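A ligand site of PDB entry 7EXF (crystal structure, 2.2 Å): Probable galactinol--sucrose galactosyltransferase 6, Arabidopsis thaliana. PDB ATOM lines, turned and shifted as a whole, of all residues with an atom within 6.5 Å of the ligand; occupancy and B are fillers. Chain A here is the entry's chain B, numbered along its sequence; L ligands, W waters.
The side-chain carboxylate (OD2) of Asp 383 sits at hydrogen-bond distance from an oxygen (O1) of the ligand (3.1 Å). SG of Cys 425 lies within hydrogen-bond range of O2 of the ligand (3.2 Å). SD of Met 426 lies within hydrogen-bond range of O1 of the ligand (2.8 Å). NE1 of Trp 307 lies within hydrogen-bond range of O4 of the ligand. An oxygen (O6) of the ligand sits at hydrogen-bond distance from the side-chain carboxylate (OD2) of Asp 244 (3.1 Å). The side-chain amino group (NZ) of Lys 381 sits at hydrogen-bond distance from an oxygen (O3) of the ligand. The side-chain carboxylate (OD2) of Asp 243 is in hydrogen-bond range of an oxygen (O4) of the ligand, at 2.6 Å. OD1 of Asp 447 sits at hydrogen-bond distance from O2 of the ligand, at 2.5 Å. The guanidinium group of Arg 443 lies within hydrogen-bond range of an oxygen (O2) of the ligand (2.8 Å).
The side-chain carboxylate of Asp 383 lies within hydrogen-bond range of the side-chain sulfur of Cys 425, at 3.2 Å. The side-chain amino group (NZ) of Lys 381 is in salt-bridge range of the side-chain carboxylate (OD1) of Asp 243, at 2.8 Å. The side-chain hydroxyl (OH) of Tyr 313 sits at hydrogen-bond distance from the side-chain carboxylate (OD1) of Asp 244 (2.6 Å). OD2 of Asp 383 sits at hydrogen-bond distance from NE1 of Trp 307, 2.8 Å away. The guanidinium group (NH1) of Arg 443 is in salt-bridge range of the side-chain carboxylate (OD1) of Asp 479. NH2 of Arg 443 sits at hydrogen-bond distance from O of Ser 445 (2.9 Å). The indole nitrogen (NE1) of Trp 314 sits at hydrogen-bond distance from the side-chain carboxylate (OD2) of Asp 244, 2.9 Å away. The guanidinium group (NH2) of Arg 443 is in salt-bridge range of the side-chain carboxylate (OD1) of Asp 447, 2.9 Å away.
Trp 211 touches the ligand. Trp 314 touches the ligand (CZ2 to O6, 3.4 Å). Met 480 touches the ligand. Hydrophobic or aromatic side chains within 4 Å of the ligand: Trp 211, Trp 307, Trp 314, Met 426 and Met 480. 12 residues have an atom within 4 Å of the ligand: Trp 211, Asp 243, Asp 244, Trp 307, Trp 314, Lys 381, Asp 383, Cys 425, Met 426, Arg 443, Asp 447 and Met 480. The nearest printed residue that does not touch the ligand is Trp 78 (4.2 Å).
Water W1 lies within hydrogen-bond range of O3 of the ligand, OD2 of Asp 479, NH1 of Arg 443 and OD1 of Asp 447. Water W2 lies within hydrogen-bond range of O1 of the ligand, OD1 of Asp 447, NE1 of Trp 78 and SD of Met 426.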
ATOM      1  N   TRP A  78      -7.859  27.922   8.224  1.00  0.00           N
ATOM      2  CA  TRP A  78      -6.751  27.234   8.912  1.00  0.00           C
ATOM      3  C   TRP A  78      -6.657  27.645  10.359  1.00  0.00           C
ATOM      4  O   TRP A  78      -6.877  28.831  10.692  1.00  0.00           O
ATOM      5  CB  TRP A  78      -5.414  27.644   8.306  1.00  0.00           C
ATOM      6  CG  TRP A  78      -5.202  27.304   6.867  1.00  0.00           C
ATOM      7  CD1 TRP A  78      -4.859  28.158   5.870  1.00  0.00           C
ATOM      8  CD2 TRP A  78      -5.311  26.017   6.259  1.00  0.00           C
ATOM      9  NE1 TRP A  78      -4.750  27.493   4.693  1.00  0.00           N
ATOM     10  CE2 TRP A  78      -4.993  26.163   4.910  1.00  0.00           C
ATOM     11  CE3 TRP A  78      -5.628  24.741   6.750  1.00  0.00           C
ATOM     12  CZ2 TRP A  78      -5.033  25.098   4.000  1.00  0.00           C
ATOM     13  CZ3 TRP A  78      -5.651  23.696   5.871  1.00  0.00           C
ATOM     14  CH2 TRP A  78      -5.311  23.874   4.504  1.00  0.00           C
ATOM     15  N   CYS A 209       3.188  16.107  -5.798  1.00  0.00           N
ATOM     16  CA  CYS A 209       2.108  17.031  -6.083  1.00  0.00           C
ATOM     17  C   CYS A 209       2.725  18.173  -6.907  1.00  0.00           C
ATOM     18  O   CYS A 209       3.786  18.643  -6.589  1.00  0.00           O
ATOM     19  CB  CYS A 209       1.556  17.557  -4.775  1.00  0.00           C
ATOM     20  SG  CYS A 209       0.406  18.938  -4.928  1.00  0.00           S
ATOM     21  N   TRP A 211       1.810  21.219  -7.377  1.00  0.00           N
ATOM     22  CA  TRP A 211       1.577  22.621  -6.986  1.00  0.00           C
ATOM     23  C   TRP A 211       2.802  23.540  -6.951  1.00  0.00           C
ATOM     24  O   TRP A 211       2.823  24.530  -7.685  1.00  0.00           O
ATOM     25  CB  TRP A 211       0.881  22.674  -5.653  1.00  0.00           C
ATOM     26  CG  TRP A 211       0.601  24.027  -5.162  1.00  0.00           C
ATOM     27  CD1 TRP A 211       0.997  24.564  -3.979  1.00  0.00           C
ATOM     28  CD2 TRP A 211      -0.092  25.051  -5.853  1.00  0.00           C
ATOM     29  NE1 TRP A 211       0.576  25.849  -3.875  1.00  0.00           N
ATOM     30  CE2 TRP A 211      -0.133  26.159  -5.019  1.00  0.00           C
ATOM     31  CE3 TRP A 211      -0.734  25.119  -7.114  1.00  0.00           C
ATOM     32  CZ2 TRP A 211      -0.776  27.361  -5.385  1.00  0.00           C
ATOM     33  CZ3 TRP A 211      -1.364  26.296  -7.489  1.00  0.00           C
ATOM     34  CH2 TRP A 211      -1.363  27.402  -6.626  1.00  0.00           C
ATOM     35  N   GLN A 216      -0.337  27.102 -11.283  1.00  0.00           N
ATOM     36  CA  GLN A 216      -1.400  26.902 -12.256  1.00  0.00           C
ATOM     37  C   GLN A 216      -0.943  26.637 -13.673  1.00  0.00           C
ATOM     38  O   GLN A 216      -1.755  26.237 -14.532  1.00  0.00           O
ATOM     39  CB  GLN A 216      -2.346  28.099 -12.295  1.00  0.00           C
ATOM     40  CG  GLN A 216      -2.958  28.477 -10.962  1.00  0.00           C
ATOM     41  CD  GLN A 216      -2.085  29.420 -10.122  1.00  0.00           C
ATOM     42  OE1 GLN A 216      -0.862  29.563 -10.354  1.00  0.00           O
ATOM     43  NE2 GLN A 216      -2.692  30.078  -9.158  1.00  0.00           N
ATOM     44  N   ASP A 243      -2.363  19.153  -9.256  1.00  0.00           N
ATOM     45  CA  ASP A 243      -3.010  20.210  -8.457  1.00  0.00           C
ATOM     46  C   ASP A 243      -3.670  21.245  -9.346  1.00  0.00           C
ATOM     47  O   ASP A 243      -3.783  21.030 -10.552  1.00  0.00           O
ATOM     48  CB  ASP A 243      -1.996  20.838  -7.490  1.00  0.00           C
ATOM     49  CG  ASP A 243      -2.606  21.255  -6.174  1.00  0.00           C
ATOM     50  OD1 ASP A 243      -2.564  20.452  -5.227  1.00  0.00           O
ATOM     51  OD2 ASP A 243      -3.133  22.376  -6.098  1.00  0.00           O
ATOM     52  N   ASP A 244      -4.059  22.355  -8.705  1.00  0.00           N
ATOM     53  CA  ASP A 244      -4.741  23.478  -9.386  1.00  0.00           C
ATOM     54  C   ASP A 244      -4.056  23.873 -10.686  1.00  0.00           C
ATOM     55  O   ASP A 244      -2.840  24.118 -10.672  1.00  0.00           O
ATOM     56  CB  ASP A 244      -4.848  24.668  -8.417  1.00  0.00           C
ATOM     57  CG  ASP A 244      -5.536  25.899  -8.973  1.00  0.00           C
ATOM     58  OD1 ASP A 244      -5.956  25.869 -10.138  1.00  0.00           O
ATOM     59  OD2 ASP A 244      -5.640  26.881  -8.231  1.00  0.00           O
ATOM     60  N   TRP A 307      -6.873  17.965  -8.072  1.00  0.00           N
ATOM     61  CA  TRP A 307      -7.417  19.078  -7.278  1.00  0.00           C
ATOM     62  C   TRP A 307      -8.748  19.658  -7.826  1.00  0.00           C
ATOM     63  O   TRP A 307      -8.908  19.816  -9.087  1.00  0.00           O
ATOM     64  CB  TRP A 307      -6.400  20.200  -7.305  1.00  0.00           C
ATOM     65  CG  TRP A 307      -6.669  21.350  -6.444  1.00  0.00           C
ATOM     66  CD1 TRP A 307      -6.169  21.556  -5.215  1.00  0.00           C
ATOM     67  CD2 TRP A 307      -7.476  22.464  -6.752  1.00  0.00           C
ATOM     68  NE1 TRP A 307      -6.605  22.755  -4.708  1.00  0.00           N
ATOM     69  CE2 TRP A 307      -7.425  23.332  -5.642  1.00  0.00           C
ATOM     70  CE3 TRP A 307      -8.199  22.859  -7.880  1.00  0.00           C
ATOM     71  CZ2 TRP A 307      -8.088  24.556  -5.622  1.00  0.00           C
ATOM     72  CZ3 TRP A 307      -8.871  24.056  -7.849  1.00  0.00           C
ATOM     73  CH2 TRP A 307      -8.809  24.892  -6.756  1.00  0.00           C
ATOM     74  N   TYR A 313     -14.241  25.746  -8.779  1.00  0.00           N
ATOM     75  CA  TYR A 313     -13.074  26.551  -8.822  1.00  0.00           C
ATOM     76  C   TYR A 313     -13.212  27.680  -7.824  1.00  0.00           C
ATOM     77  O   TYR A 313     -14.245  27.782  -7.135  1.00  0.00           O
ATOM     78  CB  TYR A 313     -12.768  27.045 -10.227  1.00  0.00           C
ATOM     79  CG  TYR A 313     -11.269  27.326 -10.430  1.00  0.00           C
ATOM     80  CD1 TYR A 313     -10.336  26.281 -10.375  1.00  0.00           C
ATOM     81  CD2 TYR A 313     -10.775  28.621 -10.672  1.00  0.00           C
ATOM     82  CE1 TYR A 313      -8.971  26.506 -10.552  1.00  0.00           C
ATOM     83  CE2 TYR A 313      -9.392  28.868 -10.832  1.00  0.00           C
ATOM     84  CZ  TYR A 313      -8.492  27.788 -10.767  1.00  0.00           C
ATOM     85  OH  TYR A 313      -7.138  27.980 -10.955  1.00  0.00           O
ATOM     86  N   TRP A 314     -12.128  28.452  -7.666  1.00  0.00           N
ATOM     87  CA  TRP A 314     -12.018  29.601  -6.759  1.00  0.00           C
ATOM     88  C   TRP A 314     -13.214  30.549  -6.853  1.00  0.00           C
ATOM     89  O   TRP A 314     -13.777  30.923  -5.825  1.00  0.00           O
ATOM     90  CB  TRP A 314     -10.696  30.343  -7.089  1.00  0.00           C
ATOM     91  CG  TRP A 314      -9.450  29.569  -6.628  1.00  0.00           C
ATOM     92  CD1 TRP A 314      -8.574  28.860  -7.392  1.00  0.00           C
ATOM     93  CD2 TRP A 314      -9.002  29.419  -5.281  1.00  0.00           C
ATOM     94  NE1 TRP A 314      -7.598  28.280  -6.611  1.00  0.00           N
ATOM     95  CE2 TRP A 314      -7.828  28.634  -5.306  1.00  0.00           C
ATOM     96  CE3 TRP A 314      -9.457  29.893  -4.061  1.00  0.00           C
ATOM     97  CZ2 TRP A 314      -7.109  28.322  -4.176  1.00  0.00           C
ATOM     98  CZ3 TRP A 314      -8.747  29.552  -2.906  1.00  0.00           C
ATOM     99  CH2 TRP A 314      -7.576  28.759  -2.989  1.00  0.00           C
ATOM    100  N   LYS A 381      -8.306  16.072  -4.282  1.00  0.00           N
ATOM    101  CA  LYS A 381      -7.912  16.928  -3.200  1.00  0.00           C
ATOM    102  C   LYS A 381      -8.978  17.982  -3.279  1.00  0.00           C
ATOM    103  O   LYS A 381      -8.948  18.780  -4.204  1.00  0.00           O
ATOM    104  CB  LYS A 381      -6.517  17.535  -3.471  1.00  0.00           C
ATOM    105  CG  LYS A 381      -6.017  18.491  -2.454  1.00  0.00           C
ATOM    106  CD  LYS A 381      -4.641  19.012  -2.834  1.00  0.00           C
ATOM    107  CE  LYS A 381      -4.175  20.193  -1.994  1.00  0.00           C
ATOM    108  NZ  LYS A 381      -2.858  20.664  -2.488  1.00  0.00           N
ATOM    109  N   ASP A 383     -10.629  21.337  -2.113  1.00  0.00           N
ATOM    110  CA  ASP A 383     -10.025  22.493  -1.442  1.00  0.00           C
ATOM    111  C   ASP A 383     -11.051  23.633  -1.277  1.00  0.00           C
ATOM    112  O   ASP A 383     -12.188  23.511  -1.673  1.00  0.00           O
ATOM    113  CB  ASP A 383      -8.891  22.963  -2.325  1.00  0.00           C
ATOM    114  CG  ASP A 383      -7.797  23.749  -1.588  1.00  0.00           C
ATOM    115  OD1 ASP A 383      -7.858  24.012  -0.374  1.00  0.00           O
ATOM    116  OD2 ASP A 383      -6.848  24.135  -2.321  1.00  0.00           O
ATOM    117  N   VAL A 384     -10.609  24.711  -0.647  1.00  0.00           N
ATOM    118  CA  VAL A 384     -11.378  25.928  -0.452  1.00  0.00           C
ATOM    119  C   VAL A 384     -12.647  25.627   0.324  1.00  0.00           C
ATOM    120  O   VAL A 384     -13.663  26.261   0.102  1.00  0.00           O
ATOM    121  CB  VAL A 384     -11.795  26.561  -1.790  1.00  0.00           C
ATOM    122  CG1 VAL A 384     -12.005  28.039  -1.618  1.00  0.00           C
ATOM    123  CG2 VAL A 384     -10.722  26.334  -2.882  1.00  0.00           C
ATOM    124  N   CYS A 425      -8.966  19.991   2.182  1.00  0.00           N
ATOM    125  CA  CYS A 425      -7.982  21.071   2.221  1.00  0.00           C
ATOM    126  C   CYS A 425      -8.729  22.418   2.466  1.00  0.00           C
ATOM    127  O   CYS A 425      -9.882  22.572   2.119  1.00  0.00           O
ATOM    128  CB  CYS A 425      -7.091  21.035   0.967  1.00  0.00           C
ATOM    129  SG  CYS A 425      -5.681  22.131   1.025  1.00  0.00           S
ATOM    130  N   MET A 426      -8.070  23.324   3.196  1.00  0.00           N
ATOM    131  CA  MET A 426      -8.622  24.586   3.622  1.00  0.00           C
ATOM    132  C   MET A 426      -9.980  24.338   4.315  1.00  0.00           C
ATOM    133  O   MET A 426     -10.990  24.958   4.000  1.00  0.00           O
ATOM    134  CB  MET A 426      -8.769  25.525   2.430  1.00  0.00           C
ATOM    135  CG  MET A 426      -7.483  26.129   1.907  1.00  0.00           C
ATOM    136  SD  MET A 426      -7.778  27.106   0.416  1.00  0.00           S
ATOM    137  CE  MET A 426      -7.410  28.770   0.914  1.00  0.00           C
ATOM    138  N   ARG A 443      -5.732  18.043   5.336  1.00  0.00           N
ATOM    139  CA  ARG A 443      -4.604  18.980   5.499  1.00  0.00           C
ATOM    140  C   ARG A 443      -4.678  19.650   6.869  1.00  0.00           C
ATOM    141  O   ARG A 443      -5.716  20.229   7.260  1.00  0.00           O
ATOM    142  CB  ARG A 443      -4.557  20.029   4.366  1.00  0.00           C
ATOM    143  CG  ARG A 443      -3.756  19.555   3.134  1.00  0.00           C
ATOM    144  CD  ARG A 443      -2.248  19.756   3.285  1.00  0.00           C
ATOM    145  NE  ARG A 443      -2.007  21.165   3.561  1.00  0.00           N
ATOM    146  CZ  ARG A 443      -2.107  22.111   2.634  1.00  0.00           C
ATOM    147  NH1 ARG A 443      -2.406  21.843   1.375  1.00  0.00           N
ATOM    148  NH2 ARG A 443      -2.006  23.346   3.002  1.00  0.00           N
ATOM    149  N   SER A 445      -2.647  22.004   8.157  1.00  0.00           N
ATOM    150  CA  SER A 445      -2.111  23.324   8.231  1.00  0.00           C
ATOM    151  C   SER A 445      -2.098  24.047   6.907  1.00  0.00           C
ATOM    152  O   SER A 445      -2.286  23.469   5.881  1.00  0.00           O
ATOM    153  CB  SER A 445      -0.682  23.334   8.780  1.00  0.00           C
ATOM    154  OG  SER A 445       0.236  22.922   7.778  1.00  0.00           O
ATOM    155  N   ASP A 446      -1.921  25.361   7.014  1.00  0.00           N
ATOM    156  CA  ASP A 446      -1.592  26.271   5.966  1.00  0.00           C
ATOM    157  C   ASP A 446      -0.414  25.713   5.176  1.00  0.00           C
ATOM    158  O   ASP A 446       0.386  24.927   5.710  1.00  0.00           O
ATOM    159  CB  ASP A 446      -1.202  27.609   6.629  1.00  0.00           C
ATOM    160  CG  ASP A 446      -1.170  28.801   5.661  1.00  0.00           C
ATOM    161  OD1 ASP A 446      -1.475  28.609   4.473  1.00  0.00           O
ATOM    162  OD2 ASP A 446      -0.831  29.926   6.115  1.00  0.00           O
ATOM    163  N   ASP A 447      -0.324  26.155   3.930  1.00  0.00           N
ATOM    164  CA  ASP A 447       0.577  25.624   2.908  1.00  0.00           C
ATOM    165  C   ASP A 447       2.024  25.698   3.300  1.00  0.00           C
ATOM    166  O   ASP A 447       2.438  26.659   3.924  1.00  0.00           O
ATOM    167  CB  ASP A 447       0.504  26.438   1.626  1.00  0.00           C
ATOM    168  CG  ASP A 447      -0.887  26.450   0.974  1.00  0.00           C
ATOM    169  OD1 ASP A 447      -1.892  25.866   1.499  1.00  0.00           O
ATOM    170  OD2 ASP A 447      -0.958  27.134  -0.093  1.00  0.00           O
ATOM    171  N   ASP A 479       1.290  18.019   4.570  1.00  0.00           N
ATOM    172  CA  ASP A 479       1.531  18.698   3.297  1.00  0.00           C
ATOM    173  C   ASP A 479       2.838  18.311   2.549  1.00  0.00           C
ATOM    174  O   ASP A 479       3.754  17.590   3.029  1.00  0.00           O
ATOM    175  CB  ASP A 479       1.454  20.232   3.456  1.00  0.00           C
ATOM    176  CG  ASP A 479       1.047  20.957   2.200  1.00  0.00           C
ATOM    177  OD1 ASP A 479       0.606  20.309   1.203  1.00  0.00           O
ATOM    178  OD2 ASP A 479       1.166  22.191   2.255  1.00  0.00           O
ATOM    179  N   MET A 480       2.871  18.768   1.332  1.00  0.00           N
ATOM    180  CA  MET A 480       4.068  18.753   0.521  1.00  0.00           C
ATOM    181  C   MET A 480       5.207  19.585   1.106  1.00  0.00           C
ATOM    182  O   MET A 480       5.032  20.408   2.014  1.00  0.00           O
ATOM    183  CB  MET A 480       3.727  19.201  -0.927  1.00  0.00           C
ATOM    184  CG  MET A 480       3.421  20.655  -1.059  1.00  0.00           C
ATOM    185  SD  MET A 480       2.518  21.121  -2.554  1.00  0.00           S
ATOM    186  CE  MET A 480       0.831  20.770  -2.057  1.00  0.00           C
ATOM    187  N   TYR A 503       4.649  13.370   0.650  1.00  0.00           N
ATOM    188  CA  TYR A 503       4.856  13.784  -0.695  1.00  0.00           C
ATOM    189  C   TYR A 503       5.613  15.078  -0.824  1.00  0.00           C
ATOM    190  O   TYR A 503       5.566  15.909   0.030  1.00  0.00           O
ATOM    191  CB  TYR A 503       3.502  13.813  -1.394  1.00  0.00           C
ATOM    192  CG  TYR A 503       2.364  14.695  -0.811  1.00  0.00           C
ATOM    193  CD1 TYR A 503       1.619  14.312   0.290  1.00  0.00           C
ATOM    194  CD2 TYR A 503       1.937  15.822  -1.470  1.00  0.00           C
ATOM    195  CE1 TYR A 503       0.534  15.068   0.776  1.00  0.00           C
ATOM    196  CE2 TYR A 503       0.863  16.614  -1.001  1.00  0.00           C
ATOM    197  CZ  TYR A 503       0.144  16.213   0.119  1.00  0.00           C
ATOM    198  OH  TYR A 503      -0.907  16.978   0.565  1.00  0.00           O
HETATM  199  C1  LIG L   1      -4.164  25.855  -1.411  1.00  0.00           C
HETATM  200  C2  LIG L   1      -3.695  24.446  -1.100  1.00  0.00           C
HETATM  201  C3  LIG L   1      -2.425  24.201  -1.869  1.00  0.00           C
HETATM  202  C4  LIG L   1      -2.800  24.192  -3.344  1.00  0.00           C
HETATM  203  C5  LIG L   1      -3.407  25.563  -3.656  1.00  0.00           C
HETATM  204  C6  LIG L   1      -3.911  25.706  -5.111  1.00  0.00           C
HETATM  205  O1  LIG L   1      -5.332  26.186  -0.630  1.00  0.00           O
HETATM  206  O2  LIG L   1      -3.411  24.245   0.252  1.00  0.00           O
HETATM  207  O3  LIG L   1      -1.831  23.007  -1.368  1.00  0.00           O
HETATM  208  O4  LIG L   1      -3.731  23.152  -3.698  1.00  0.00           O
HETATM  209  O5  LIG L   1      -4.519  25.805  -2.783  1.00  0.00           O
HETATM  210  O6  LIG L   1      -4.261  27.094  -5.450  1.00  0.00           O
HETATM  211  O   HOH W   1       0.154  23.508   0.036  1.00  0.00           O
HETATM  212  O   HOH W   2      -4.310  27.421   1.489  1.00  0.00           O
